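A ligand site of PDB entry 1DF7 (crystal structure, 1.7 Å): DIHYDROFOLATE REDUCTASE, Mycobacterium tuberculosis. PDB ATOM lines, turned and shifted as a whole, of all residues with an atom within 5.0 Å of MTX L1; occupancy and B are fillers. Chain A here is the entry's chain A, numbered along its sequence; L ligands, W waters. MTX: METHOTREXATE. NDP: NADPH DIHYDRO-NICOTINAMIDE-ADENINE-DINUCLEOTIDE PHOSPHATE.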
ATOM      1  N   ILE A   5      11.754 -22.468 -18.730  1.00  0.00           N
ATOM      2  CA  ILE A   5      10.546 -22.510 -19.569  1.00  0.00           C
ATOM      3  C   ILE A   5      10.973 -22.711 -21.023  1.00  0.00           C
ATOM      4  O   ILE A   5      11.875 -22.025 -21.519  1.00  0.00           O
ATOM      5  CB  ILE A   5       9.681 -21.262 -19.394  1.00  0.00           C
ATOM      6  CG1 ILE A   5       8.447 -21.346 -20.295  1.00  0.00           C
ATOM      7  CG2 ILE A   5      10.480 -20.023 -19.676  1.00  0.00           C
ATOM      8  CD1 ILE A   5       7.412 -20.268 -20.007  1.00  0.00           C
ATOM      9  N   TRP A   6      10.396 -23.700 -21.693  1.00  0.00           N
ATOM     10  CA  TRP A   6      10.741 -23.972 -23.093  1.00  0.00           C
ATOM     11  C   TRP A   6       9.573 -24.685 -23.813  1.00  0.00           C
ATOM     12  O   TRP A   6       8.666 -25.229 -23.166  1.00  0.00           O
ATOM     13  CB  TRP A   6      12.006 -24.859 -23.170  1.00  0.00           C
ATOM     14  CG  TRP A   6      11.812 -26.354 -22.823  1.00  0.00           C
ATOM     15  CD1 TRP A   6      11.378 -27.345 -23.668  1.00  0.00           C
ATOM     16  CD2 TRP A   6      12.143 -27.003 -21.585  1.00  0.00           C
ATOM     17  NE1 TRP A   6      11.428 -28.587 -23.024  1.00  0.00           N
ATOM     18  CE2 TRP A   6      11.893 -28.397 -21.752  1.00  0.00           C
ATOM     19  CE3 TRP A   6      12.653 -26.551 -20.355  1.00  0.00           C
ATOM     20  CZ2 TRP A   6      12.136 -29.327 -20.729  1.00  0.00           C
ATOM     21  CZ3 TRP A   6      12.889 -27.482 -19.339  1.00  0.00           C
ATOM     22  CH2 TRP A   6      12.619 -28.856 -19.542  1.00  0.00           C
ATOM     23  N   ALA A   7       9.623 -24.699 -25.150  1.00  0.00           N
ATOM     24  CA  ALA A   7       8.634 -25.379 -26.009  1.00  0.00           C
ATOM     25  C   ALA A   7       9.491 -26.371 -26.814  1.00  0.00           C
ATOM     26  O   ALA A   7      10.520 -25.996 -27.387  1.00  0.00           O
ATOM     27  CB  ALA A   7       7.944 -24.393 -26.947  1.00  0.00           C
ATOM     28  N   ILE A  20      13.247 -21.351 -33.871  1.00  0.00           N
ATOM     29  CA  ILE A  20      12.347 -22.363 -33.326  1.00  0.00           C
ATOM     30  C   ILE A  20      11.634 -22.873 -34.592  1.00  0.00           C
ATOM     31  O   ILE A  20      10.985 -22.095 -35.290  1.00  0.00           O
ATOM     32  CB  ILE A  20      11.399 -21.766 -32.276  1.00  0.00           C
ATOM     33  CG1 ILE A  20      12.208 -21.338 -31.052  1.00  0.00           C
ATOM     34  CG2 ILE A  20      10.351 -22.757 -31.893  1.00  0.00           C
ATOM     35  CD1 ILE A  20      11.449 -20.551 -30.064  1.00  0.00           C
ATOM     36  N   PRO A  25       1.757 -19.344 -31.870  1.00  0.00           N
ATOM     37  CA  PRO A  25       1.515 -18.097 -31.160  1.00  0.00           C
ATOM     38  C   PRO A  25       0.910 -18.271 -29.744  1.00  0.00           C
ATOM     39  O   PRO A  25       1.247 -17.508 -28.847  1.00  0.00           O
ATOM     40  CB  PRO A  25       0.615 -17.310 -32.115  1.00  0.00           C
ATOM     41  CG  PRO A  25      -0.047 -18.349 -32.913  1.00  0.00           C
ATOM     42  CD  PRO A  25       1.011 -19.398 -33.138  1.00  0.00           C
ATOM     43  N   ASP A  27       1.681 -20.496 -27.665  1.00  0.00           N
ATOM     44  CA  ASP A  27       2.783 -20.797 -26.766  1.00  0.00           C
ATOM     45  C   ASP A  27       3.501 -19.493 -26.377  1.00  0.00           C
ATOM     46  O   ASP A  27       3.983 -19.358 -25.252  1.00  0.00           O
ATOM     47  CB  ASP A  27       3.749 -21.816 -27.354  1.00  0.00           C
ATOM     48  CG  ASP A  27       5.012 -21.951 -26.515  1.00  0.00           C
ATOM     49  OD1 ASP A  27       4.917 -22.394 -25.354  1.00  0.00           O
ATOM     50  OD2 ASP A  27       6.076 -21.543 -27.024  1.00  0.00           O
ATOM     51  N   GLN A  28       3.544 -18.536 -27.292  1.00  0.00           N
ATOM     52  CA  GLN A  28       4.163 -17.260 -26.960  1.00  0.00           C
ATOM     53  C   GLN A  28       3.359 -16.507 -25.913  1.00  0.00           C
ATOM     54  O   GLN A  28       3.929 -15.852 -25.027  1.00  0.00           O
ATOM     55  CB  GLN A  28       4.312 -16.418 -28.200  1.00  0.00           C
ATOM     56  CG  GLN A  28       5.467 -16.863 -29.029  1.00  0.00           C
ATOM     57  CD  GLN A  28       5.725 -15.900 -30.121  1.00  0.00           C
ATOM     58  OE1 GLN A  28       5.074 -14.844 -30.182  1.00  0.00           O
ATOM     59  NE2 GLN A  28       6.673 -16.219 -30.979  1.00  0.00           N
ATOM     60  N   ALA A  29       2.041 -16.645 -25.985  1.00  0.00           N
ATOM     61  CA  ALA A  29       1.148 -15.999 -25.020  1.00  0.00           C
ATOM     62  C   ALA A  29       1.409 -16.613 -23.638  1.00  0.00           C
ATOM     63  O   ALA A  29       1.488 -15.912 -22.636  1.00  0.00           O
ATOM     64  CB  ALA A  29      -0.328 -16.191 -25.460  1.00  0.00           C
ATOM     65  N   HIS A  30       1.526 -17.934 -23.593  1.00  0.00           N
ATOM     66  CA  HIS A  30       1.778 -18.689 -22.376  1.00  0.00           C
ATOM     67  C   HIS A  30       3.129 -18.246 -21.776  1.00  0.00           C
ATOM     68  O   HIS A  30       3.256 -18.015 -20.572  1.00  0.00           O
ATOM     69  CB  HIS A  30       1.810 -20.185 -22.732  1.00  0.00           C
ATOM     70  CG  HIS A  30       2.287 -21.069 -21.619  1.00  0.00           C
ATOM     71  ND1 HIS A  30       1.585 -21.221 -20.446  1.00  0.00           N
ATOM     72  CD2 HIS A  30       3.381 -21.861 -21.518  1.00  0.00           C
ATOM     73  CE1 HIS A  30       2.220 -22.078 -19.665  1.00  0.00           C
ATOM     74  NE2 HIS A  30       3.308 -22.486 -20.296  1.00  0.00           N
ATOM     75  N   PHE A  31       4.124 -18.139 -22.647  1.00  0.00           N
ATOM     76  CA  PHE A  31       5.470 -17.721 -22.257  1.00  0.00           C
ATOM     77  C   PHE A  31       5.383 -16.343 -21.560  1.00  0.00           C
ATOM     78  O   PHE A  31       5.920 -16.150 -20.462  1.00  0.00           O
ATOM     79  CB  PHE A  31       6.360 -17.665 -23.508  1.00  0.00           C
ATOM     80  CG  PHE A  31       7.658 -16.930 -23.320  1.00  0.00           C
ATOM     81  CD1 PHE A  31       8.764 -17.582 -22.787  1.00  0.00           C
ATOM     82  CD2 PHE A  31       7.770 -15.592 -23.685  1.00  0.00           C
ATOM     83  CE1 PHE A  31       9.960 -16.919 -22.613  1.00  0.00           C
ATOM     84  CE2 PHE A  31       8.974 -14.904 -23.532  1.00  0.00           C
ATOM     85  CZ  PHE A  31      10.072 -15.575 -22.991  1.00  0.00           C
ATOM     86  N   ARG A  32       4.637 -15.428 -22.185  1.00  0.00           N
ATOM     87  CA  ARG A  32       4.445 -14.080 -21.653  1.00  0.00           C
ATOM     88  C   ARG A  32       3.782 -14.136 -20.291  1.00  0.00           C
ATOM     89  O   ARG A  32       4.253 -13.491 -19.346  1.00  0.00           O
ATOM     90  CB  ARG A  32       3.606 -13.253 -22.612  1.00  0.00           C
ATOM     91  CG  ARG A  32       3.346 -11.862 -22.110  1.00  0.00           C
ATOM     92  CD  ARG A  32       2.408 -11.125 -23.014  1.00  0.00           C
ATOM     93  NE  ARG A  32       2.020  -9.858 -22.382  1.00  0.00           N
ATOM     94  CZ  ARG A  32       2.625  -8.668 -22.553  1.00  0.00           C
ATOM     95  NH1 ARG A  32       3.688  -8.512 -23.364  1.00  0.00           N
ATOM     96  NH2 ARG A  32       2.152  -7.600 -21.896  1.00  0.00           N
ATOM     97  N   THR A  35       6.418 -15.509 -17.673  1.00  0.00           N
ATOM     98  CA  THR A  35       7.562 -14.648 -17.412  1.00  0.00           C
ATOM     99  C   THR A  35       7.338 -13.186 -17.060  1.00  0.00           C
ATOM    100  O   THR A  35       8.194 -12.568 -16.452  1.00  0.00           O
ATOM    101  CB  THR A  35       8.509 -14.687 -18.608  1.00  0.00           C
ATOM    102  OG1 THR A  35       7.827 -14.188 -19.762  1.00  0.00           O
ATOM    103  CG2 THR A  35       8.969 -16.123 -18.901  1.00  0.00           C
ATOM    104  N   MET A  36       6.187 -12.624 -17.434  1.00  0.00           N
ATOM    105  CA  MET A  36       5.935 -11.204 -17.197  1.00  0.00           C
ATOM    106  C   MET A  36       6.176 -10.765 -15.749  1.00  0.00           C
ATOM    107  O   MET A  36       5.849 -11.486 -14.813  1.00  0.00           O
ATOM    108  CB  MET A  36       4.512 -10.827 -17.653  1.00  0.00           C
ATOM    109  CG  MET A  36       4.219  -9.355 -17.545  1.00  0.00           C
ATOM    110  SD  MET A  36       5.184  -8.349 -18.643  1.00  0.00           S
ATOM    111  CE  MET A  36       4.746  -8.983 -20.107  1.00  0.00           C
ATOM    112  N   THR A  46      20.120 -16.985 -27.842  1.00  0.00           N
ATOM    113  CA  THR A  46      18.688 -16.796 -27.677  1.00  0.00           C
ATOM    114  C   THR A  46      18.371 -15.308 -27.758  1.00  0.00           C
ATOM    115  O   THR A  46      17.420 -14.938 -28.382  1.00  0.00           O
ATOM    116  CB  THR A  46      18.185 -17.428 -26.373  1.00  0.00           C
ATOM    117  OG1 THR A  46      18.264 -18.851 -26.505  1.00  0.00           O
ATOM    118  CG2 THR A  46      16.694 -17.046 -26.117  1.00  0.00           C
ATOM    119  N   SER A  49      18.293 -14.233 -31.306  1.00  0.00           N
ATOM    120  CA  SER A  49      17.111 -14.767 -31.966  1.00  0.00           C
ATOM    121  C   SER A  49      15.824 -14.017 -31.683  1.00  0.00           C
ATOM    122  O   SER A  49      14.819 -14.262 -32.347  1.00  0.00           O
ATOM    123  CB  SER A  49      16.904 -16.247 -31.636  1.00  0.00           C
ATOM    124  OG  SER A  49      16.356 -16.428 -30.335  1.00  0.00           O
ATOM    125  N   LEU A  50      15.796 -13.162 -30.655  1.00  0.00           N
ATOM    126  CA  LEU A  50      14.551 -12.430 -30.344  1.00  0.00           C
ATOM    127  C   LEU A  50      14.241 -11.429 -31.455  1.00  0.00           C
ATOM    128  O   LEU A  50      15.151 -10.828 -32.017  1.00  0.00           O
ATOM    129  CB  LEU A  50      14.652 -11.671 -29.006  1.00  0.00           C
ATOM    130  CG  LEU A  50      14.730 -12.517 -27.727  1.00  0.00           C
ATOM    131  CD1 LEU A  50      14.939 -11.597 -26.539  1.00  0.00           C
ATOM    132  CD2 LEU A  50      13.499 -13.355 -27.541  1.00  0.00           C
ATOM    133  N   PRO A  51      12.969 -11.347 -31.870  1.00  0.00           N
ATOM    134  CA  PRO A  51      12.707 -10.367 -32.917  1.00  0.00           C
ATOM    135  C   PRO A  51      13.025  -8.998 -32.290  1.00  0.00           C
ATOM    136  O   PRO A  51      12.841  -8.770 -31.084  1.00  0.00           O
ATOM    137  CB  PRO A  51      11.202 -10.521 -33.155  1.00  0.00           C
ATOM    138  CG  PRO A  51      10.923 -11.918 -32.791  1.00  0.00           C
ATOM    139  CD  PRO A  51      11.770 -12.135 -31.559  1.00  0.00           C
ATOM    140  N   VAL A  54      10.803  -7.094 -29.749  1.00  0.00           N
ATOM    141  CA  VAL A  54      10.693  -7.535 -28.371  1.00  0.00           C
ATOM    142  C   VAL A  54      12.038  -7.888 -27.806  1.00  0.00           C
ATOM    143  O   VAL A  54      12.176  -8.817 -27.018  1.00  0.00           O
ATOM    144  CB  VAL A  54       9.757  -8.733 -28.206  1.00  0.00           C
ATOM    145  CG1 VAL A  54       8.341  -8.325 -28.512  1.00  0.00           C
ATOM    146  CG2 VAL A  54      10.218  -9.883 -29.110  1.00  0.00           C
ATOM    147  N   LEU A  57      12.673  -8.131 -24.042  1.00  0.00           N
ATOM    148  CA  LEU A  57      11.286  -8.478 -23.817  1.00  0.00           C
ATOM    149  C   LEU A  57      10.754  -7.501 -22.802  1.00  0.00           C
ATOM    150  O   LEU A  57      11.332  -7.348 -21.732  1.00  0.00           O
ATOM    151  CB  LEU A  57      11.168  -9.925 -23.320  1.00  0.00           C
ATOM    152  CG  LEU A  57      11.339 -10.906 -24.482  1.00  0.00           C
ATOM    153  CD1 LEU A  57      11.735 -12.267 -23.979  1.00  0.00           C
ATOM    154  CD2 LEU A  57      10.036 -10.963 -25.296  1.00  0.00           C
ATOM    155  N   PRO A  58       9.669  -6.805 -23.126  1.00  0.00           N
ATOM    156  CA  PRO A  58       9.101  -5.815 -22.202  1.00  0.00           C
ATOM    157  C   PRO A  58       8.500  -6.341 -20.939  1.00  0.00           C
ATOM    158  O   PRO A  58       7.955  -7.446 -20.900  1.00  0.00           O
ATOM    159  CB  PRO A  58       8.056  -5.082 -23.067  1.00  0.00           C
ATOM    160  CG  PRO A  58       7.588  -6.163 -24.007  1.00  0.00           C
ATOM    161  CD  PRO A  58       8.908  -6.841 -24.394  1.00  0.00           C
ATOM    162  N   ARG A  60      10.038  -7.252 -18.265  1.00  0.00           N
ATOM    163  CA  ARG A  60      10.904  -8.243 -17.621  1.00  0.00           C
ATOM    164  C   ARG A  60      12.338  -7.732 -17.591  1.00  0.00           C
ATOM    165  O   ARG A  60      12.732  -6.944 -18.452  1.00  0.00           O
ATOM    166  CB  ARG A  60      10.865  -9.535 -18.417  1.00  0.00           C
ATOM    167  CG  ARG A  60       9.625 -10.386 -18.136  1.00  0.00           C
ATOM    168  CD  ARG A  60       9.125 -11.138 -19.367  1.00  0.00           C
ATOM    169  NE  ARG A  60       8.590 -10.242 -20.379  1.00  0.00           N
ATOM    170  CZ  ARG A  60       7.922 -10.628 -21.460  1.00  0.00           C
ATOM    171  NH1 ARG A  60       7.692 -11.909 -21.675  1.00  0.00           N
ATOM    172  NH2 ARG A  60       7.482  -9.710 -22.325  1.00  0.00           N
ATOM    173  N   ILE A  94      15.036 -18.771 -20.107  1.00  0.00           N
ATOM    174  CA  ILE A  94      14.237 -18.894 -21.322  1.00  0.00           C
ATOM    175  C   ILE A  94      14.979 -19.418 -22.546  1.00  0.00           C
ATOM    176  O   ILE A  94      14.479 -19.311 -23.677  1.00  0.00           O
ATOM    177  CB  ILE A  94      13.558 -17.542 -21.651  1.00  0.00           C
ATOM    178  CG1 ILE A  94      14.607 -16.503 -22.090  1.00  0.00           C
ATOM    179  CG2 ILE A  94      12.835 -17.033 -20.404  1.00  0.00           C
ATOM    180  CD1 ILE A  94      14.068 -15.464 -23.081  1.00  0.00           C
ATOM    181  N   GLY A  95      16.155 -19.996 -22.426  1.00  0.00           N
ATOM    182  CA  GLY A  95      16.827 -20.624 -23.379  1.00  0.00           C
ATOM    183  C   GLY A  95      18.399 -20.233 -23.449  1.00  0.00           C
ATOM    184  O   GLY A  95      18.822 -19.347 -22.823  1.00  0.00           O
ATOM    185  N   TYR A 100      19.945 -23.966 -20.785  1.00  0.00           N
ATOM    186  CA  TYR A 100      19.037 -24.870 -20.072  1.00  0.00           C
ATOM    187  C   TYR A 100      19.877 -25.943 -19.374  1.00  0.00           C
ATOM    188  O   TYR A 100      19.619 -26.294 -18.230  1.00  0.00           O
ATOM    189  CB  TYR A 100      18.053 -25.565 -21.022  1.00  0.00           C
ATOM    190  CG  TYR A 100      16.904 -24.704 -21.565  1.00  0.00           C
ATOM    191  CD1 TYR A 100      16.514 -24.818 -22.912  1.00  0.00           C
ATOM    192  CD2 TYR A 100      16.216 -23.793 -20.762  1.00  0.00           C
ATOM    193  CE1 TYR A 100      15.492 -24.050 -23.442  1.00  0.00           C
ATOM    194  CE2 TYR A 100      15.182 -23.011 -21.309  1.00  0.00           C
ATOM    195  CZ  TYR A 100      14.840 -23.154 -22.649  1.00  0.00           C
ATOM    196  OH  TYR A 100      13.854 -22.354 -23.216  1.00  0.00           O
ATOM    197  N   THR A 113       6.127 -26.827 -22.887  1.00  0.00           N
ATOM    198  CA  THR A 113       5.081 -26.902 -23.892  1.00  0.00           C
ATOM    199  C   THR A 113       5.534 -28.006 -24.830  1.00  0.00           C
ATOM    200  O   THR A 113       6.656 -27.933 -25.374  1.00  0.00           O
ATOM    201  CB  THR A 113       4.971 -25.600 -24.674  1.00  0.00           C
ATOM    202  OG1 THR A 113       4.571 -24.544 -23.791  1.00  0.00           O
ATOM    203  CG2 THR A 113       3.943 -25.753 -25.828  1.00  0.00           C
HETATM  204  N1  MTX L   1       8.132 -20.613 -25.664  1.00  0.00           N
HETATM  205  C2  MTX L   1       8.376 -21.195 -24.422  1.00  0.00           C
HETATM  206  NA2 MTX L   1       7.386 -21.984 -23.938  1.00  0.00           N
HETATM  207  N3  MTX L   1       9.533 -20.986 -23.770  1.00  0.00           N
HETATM  208  C4  MTX L   1      10.563 -20.219 -24.167  1.00  0.00           C
HETATM  209  NA4 MTX L   1      11.646 -20.021 -23.482  1.00  0.00           N
HETATM  210  C4A MTX L   1      10.315 -19.557 -25.461  1.00  0.00           C
HETATM  211  N5  MTX L   1      11.211 -18.677 -25.975  1.00  0.00           N
HETATM  212  C6  MTX L   1      10.937 -18.146 -27.160  1.00  0.00           C
HETATM  213  C7  MTX L   1       9.770 -18.563 -27.804  1.00  0.00           C
HETATM  214  N8  MTX L   1       8.856 -19.261 -27.396  1.00  0.00           N
HETATM  215  C8A MTX L   1       9.122 -19.836 -26.176  1.00  0.00           C
HETATM  216  C9  MTX L   1      12.057 -17.263 -27.731  1.00  0.00           C
HETATM  217  N10 MTX L   1      11.512 -16.371 -28.690  1.00  0.00           N
HETATM  218  CM  MTX L   1      12.202 -16.485 -30.040  1.00  0.00           C
HETATM  219  C11 MTX L   1       8.454 -13.596 -28.125  1.00  0.00           C
HETATM  220  C12 MTX L   1       8.976 -13.852 -29.419  1.00  0.00           C
HETATM  221  C13 MTX L   1       9.980 -14.653 -29.829  1.00  0.00           C
HETATM  222  C14 MTX L   1      10.589 -15.385 -28.618  1.00  0.00           C
HETATM  223  C15 MTX L   1      10.006 -15.117 -27.276  1.00  0.00           C
HETATM  224  C16 MTX L   1       8.983 -14.354 -27.034  1.00  0.00           C
HETATM  225  C   MTX L   1       7.432 -12.744 -28.054  1.00  0.00           C
HETATM  226  O   MTX L   1       6.842 -11.967 -28.826  1.00  0.00           O
HETATM  227  N   MTX L   1       6.689 -12.535 -27.021  1.00  0.00           N
HETATM  228  CA  MTX L   1       5.807 -11.707 -26.450  1.00  0.00           C
HETATM  229  CT  MTX L   1       6.080 -11.651 -24.955  1.00  0.00           C
HETATM  230  O1  MTX L   1       6.515 -12.447 -24.155  1.00  0.00           O
HETATM  231  O2  MTX L   1       5.732 -10.401 -24.480  1.00  0.00           O
HETATM  232  CB  MTX L   1       4.259 -12.019 -26.404  1.00  0.00           C
HETATM  233  CG  MTX L   1       3.513 -12.394 -27.635  1.00  0.00           C
HETATM  234  CD  MTX L   1       2.141 -13.286 -27.935  1.00  0.00           C
HETATM  235  OE1 MTX L   1       1.890 -14.009 -29.076  1.00  0.00           O
HETATM  236  OE2 MTX L   1       1.716 -12.904 -26.751  1.00  0.00           O
HETATM  237  PA  NDP L   2      22.111 -20.317 -26.126  1.00  0.00           P
HETATM  238  O1A NDP L   2      21.997 -21.181 -24.936  1.00  0.00           O
HETATM  239  O2A NDP L   2      20.941 -19.422 -26.345  1.00  0.00           O
HETATM  240  O5B NDP L   2      23.356 -19.338 -26.009  1.00  0.00           O
HETATM  241  C5B NDP L   2      24.670 -19.964 -25.860  1.00  0.00           C
HETATM  242  C4B NDP L   2      25.594 -18.750 -25.627  1.00  0.00           C
HETATM  243  O4B NDP L   2      25.432 -18.376 -24.255  1.00  0.00           O
HETATM  244  C3B NDP L   2      27.091 -19.108 -25.774  1.00  0.00           C
HETATM  245  O3B NDP L   2      27.379 -19.078 -27.168  1.00  0.00           O
HETATM  246  C2B NDP L   2      27.673 -17.959 -24.878  1.00  0.00           C
HETATM  247  O2B NDP L   2      27.653 -16.672 -25.437  1.00  0.00           O
HETATM  248  C1B NDP L   2      26.731 -18.021 -23.716  1.00  0.00           C
HETATM  249  N9A NDP L   2      27.149 -18.985 -22.715  1.00  0.00           N
HETATM  250  C8A NDP L   2      26.933 -20.334 -22.660  1.00  0.00           C
HETATM  251  N7A NDP L   2      27.441 -20.901 -21.572  1.00  0.00           N
HETATM  252  C5A NDP L   2      28.003 -19.836 -20.900  1.00  0.00           C
HETATM  253  C6A NDP L   2      28.725 -19.757 -19.635  1.00  0.00           C
HETATM  254  N6A NDP L   2      28.955 -20.875 -18.887  1.00  0.00           N
HETATM  255  N1A NDP L   2      29.148 -18.512 -19.260  1.00  0.00           N
HETATM  256  C2A NDP L   2      28.889 -17.444 -20.080  1.00  0.00           C
HETATM  257  N3A NDP L   2      28.255 -17.419 -21.233  1.00  0.00           N
HETATM  258  C4A NDP L   2      27.821 -18.657 -21.581  1.00  0.00           C
HETATM  259  O3  NDP L   2      22.366 -21.126 -27.385  1.00  0.00           O
HETATM  260  PN  NDP L   2      21.970 -22.493 -28.088  1.00  0.00           P
HETATM  261  O1N NDP L   2      22.619 -22.625 -29.411  1.00  0.00           O
HETATM  262  O2N NDP L   2      22.233 -23.641 -27.218  1.00  0.00           O
HETATM  263  O5D NDP L   2      20.341 -22.328 -28.238  1.00  0.00           O
HETATM  264  C5D NDP L   2      19.854 -21.381 -29.240  1.00  0.00           C
HETATM  265  C4D NDP L   2      18.743 -22.162 -29.962  1.00  0.00           C
HETATM  266  O4D NDP L   2      17.692 -22.401 -28.979  1.00  0.00           O
HETATM  267  C3D NDP L   2      18.058 -21.380 -31.122  1.00  0.00           C
HETATM  268  O3D NDP L   2      17.849 -22.269 -32.167  1.00  0.00           O
HETATM  269  C2D NDP L   2      16.763 -20.895 -30.465  1.00  0.00           C
HETATM  270  O2D NDP L   2      15.789 -20.687 -31.482  1.00  0.00           O
HETATM  271  C1D NDP L   2      16.418 -22.036 -29.530  1.00  0.00           C
HETATM  272  N1N NDP L   2      15.500 -21.649 -28.401  1.00  0.00           N
HETATM  273  C2N NDP L   2      14.309 -22.416 -28.312  1.00  0.00           C
HETATM  274  C3N NDP L   2      13.436 -22.105 -27.287  1.00  0.00           C
HETATM  275  C7N NDP L   2      12.113 -22.959 -27.207  1.00  0.00           C
HETATM  276  O7N NDP L   2      11.470 -22.840 -26.220  1.00  0.00           O
HETATM  277  N7N NDP L   2      11.790 -23.786 -28.263  1.00  0.00           N
HETATM  278  C4N NDP L   2      13.652 -21.068 -26.305  1.00  0.00           C
HETATM  279  C5N NDP L   2      14.896 -20.374 -26.520  1.00  0.00           C
HETATM  280  C6N NDP L   2      15.795 -20.624 -27.500  1.00  0.00           C
HETATM  281  P2B NDP L   2      28.957 -16.135 -26.374  1.00  0.00           P
HETATM  282  O1X NDP L   2      29.009 -17.012 -27.513  1.00  0.00           O
HETATM  283  O2X NDP L   2      28.397 -14.751 -26.638  1.00  0.00           O
HETATM  284  O3X NDP L   2      30.068 -16.238 -25.409  1.00  0.00           O
HETATM  285  O   HOH W   1      14.553 -18.444 -30.813  1.00  0.00           O
HETATM  286  O   HOH W   2       6.997 -11.062 -31.328  1.00  0.00           O
HETATM  287  O   HOH W   3      -1.205 -12.937 -27.628  1.00  0.00           O
HETATM  288  O   HOH W   4       4.828  -8.370 -25.883  1.00  0.00           O
HETATM  289  O   HOH W   5       6.102 -23.589 -21.723  1.00  0.00           O
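OE1 of MTX L1 sits close to OE1 of Gln 28, at 3.5 Å. A nitrogen (NA4) of MTX L1 is in hydrogen-bond range of the backbone carbonyl oxygen of Ile 5 (2.8 Å). OG1 of Thr 46 is in hydrogen-bond range of O2A of NDP L2 (2.7 Å). A nitrogen (N1) of MTX L1 lies within hydrogen-bond range of the side-chain carboxylate (OD2) of Asp 27 (2.6 Å). An oxygen (O2) of MTX L1 is in salt-bridge range of the guanidinium group (NH1) of Arg 32, at 3.0 Å. The backbone carbonyl oxygen (O) of Ala 7 is in hydrogen-bond range of a nitrogen (N7N) of NDP L2, 2.7 Å away. O2A of NDP L2 is in hydrogen-bond range of N of Thr 46, 3.0 Å away. N of Ala 7 sits at hydrogen-bond distance from O7N of NDP L2, at 2.8 Å. The backbone carbonyl oxygen (O) of Ile 94 lies within hydrogen-bond range of a nitrogen (NA4) of MTX L1 (2.9 Å). The side-chain hydroxyl (OH) of Tyr 100 sits at hydrogen-bond distance from a nitrogen (NA4) of MTX L1 (3.2 Å). The guanidinium group (NH1) of Arg 60 lies within salt-bridge range of an oxygen (O1) of MTX L1 (2.8 Å).
O of Trp 6 is in hydrogen-bond range of N of Thr 113 (3.0 Å). The backbone carbonyl oxygen (O) of Ile 5 lies within hydrogen-bond range of the side-chain hydroxyl (OH) of Tyr 100, at 2.6 Å. The side-chain hydroxyl (OH) of Tyr 100 lies within hydrogen-bond range of the backbone carbonyl oxygen (O) of Ile 94 (3.1 Å). The side-chain carboxylate of Asp 27 is in hydrogen-bond range of the side-chain hydroxyl of Thr 113 (2.7 Å). The backbone carbonyl oxygen (O) of Phe 31 lies within hydrogen-bond range of the side-chain hydroxyl (OG1) of Thr 35 (2.8 Å). NH1 of Arg 60 lies within hydrogen-bond range of OG1 of Thr 35, at 3.0 Å. The backbone carbonyl oxygen (O) of Pro 58 lies within hydrogen-bond range of the guanidinium group (NH2) of Arg 60 (2.7 Å). The side-chain hydroxyl (OH) of Tyr 100 lies close to the backbone NH (N) of Gly 95 (3.4 Å).
Merely in contact with MTX L1: Trp 6, Phe 31, Ile 20, Pro 51, Pro 25, Ala 29, Leu 50, Ala 7, Thr 113, Val 54 and Leu 57. 18 residues have an atom within 4 Å of MTX L1: Ile 5, Trp 6, Ala 7, Ile 20, Pro 25, Asp 27, Gln 28, Ala 29, Phe 31, Arg 32, Leu 50, Pro 51, Val 54, Leu 57, Arg 60, Ile 94, Tyr 100 and Thr 113. The nearest printed residue that does not touch MTX L1 is Ser 49 (4.1 Å).
Water W4 lies within hydrogen-bond range of an oxygen (O2) of MTX L1 and the guanidinium group (NH1) of Arg 32. Water W5 lies within hydrogen-bond range of the side-chain hydroxyl of Thr 113 (2.7 Å), a nitrogen (NA2) of MTX L1 (3.0 Å), a ring nitrogen (NE2) of His 30 (3.3 Å) and the backbone carbonyl oxygen of Trp 6 (3.4 Å). Water W1 lies within hydrogen-bond range of O2D of NDP L2 (2.6 Å) and OG of Ser 49 (2.7 Å).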
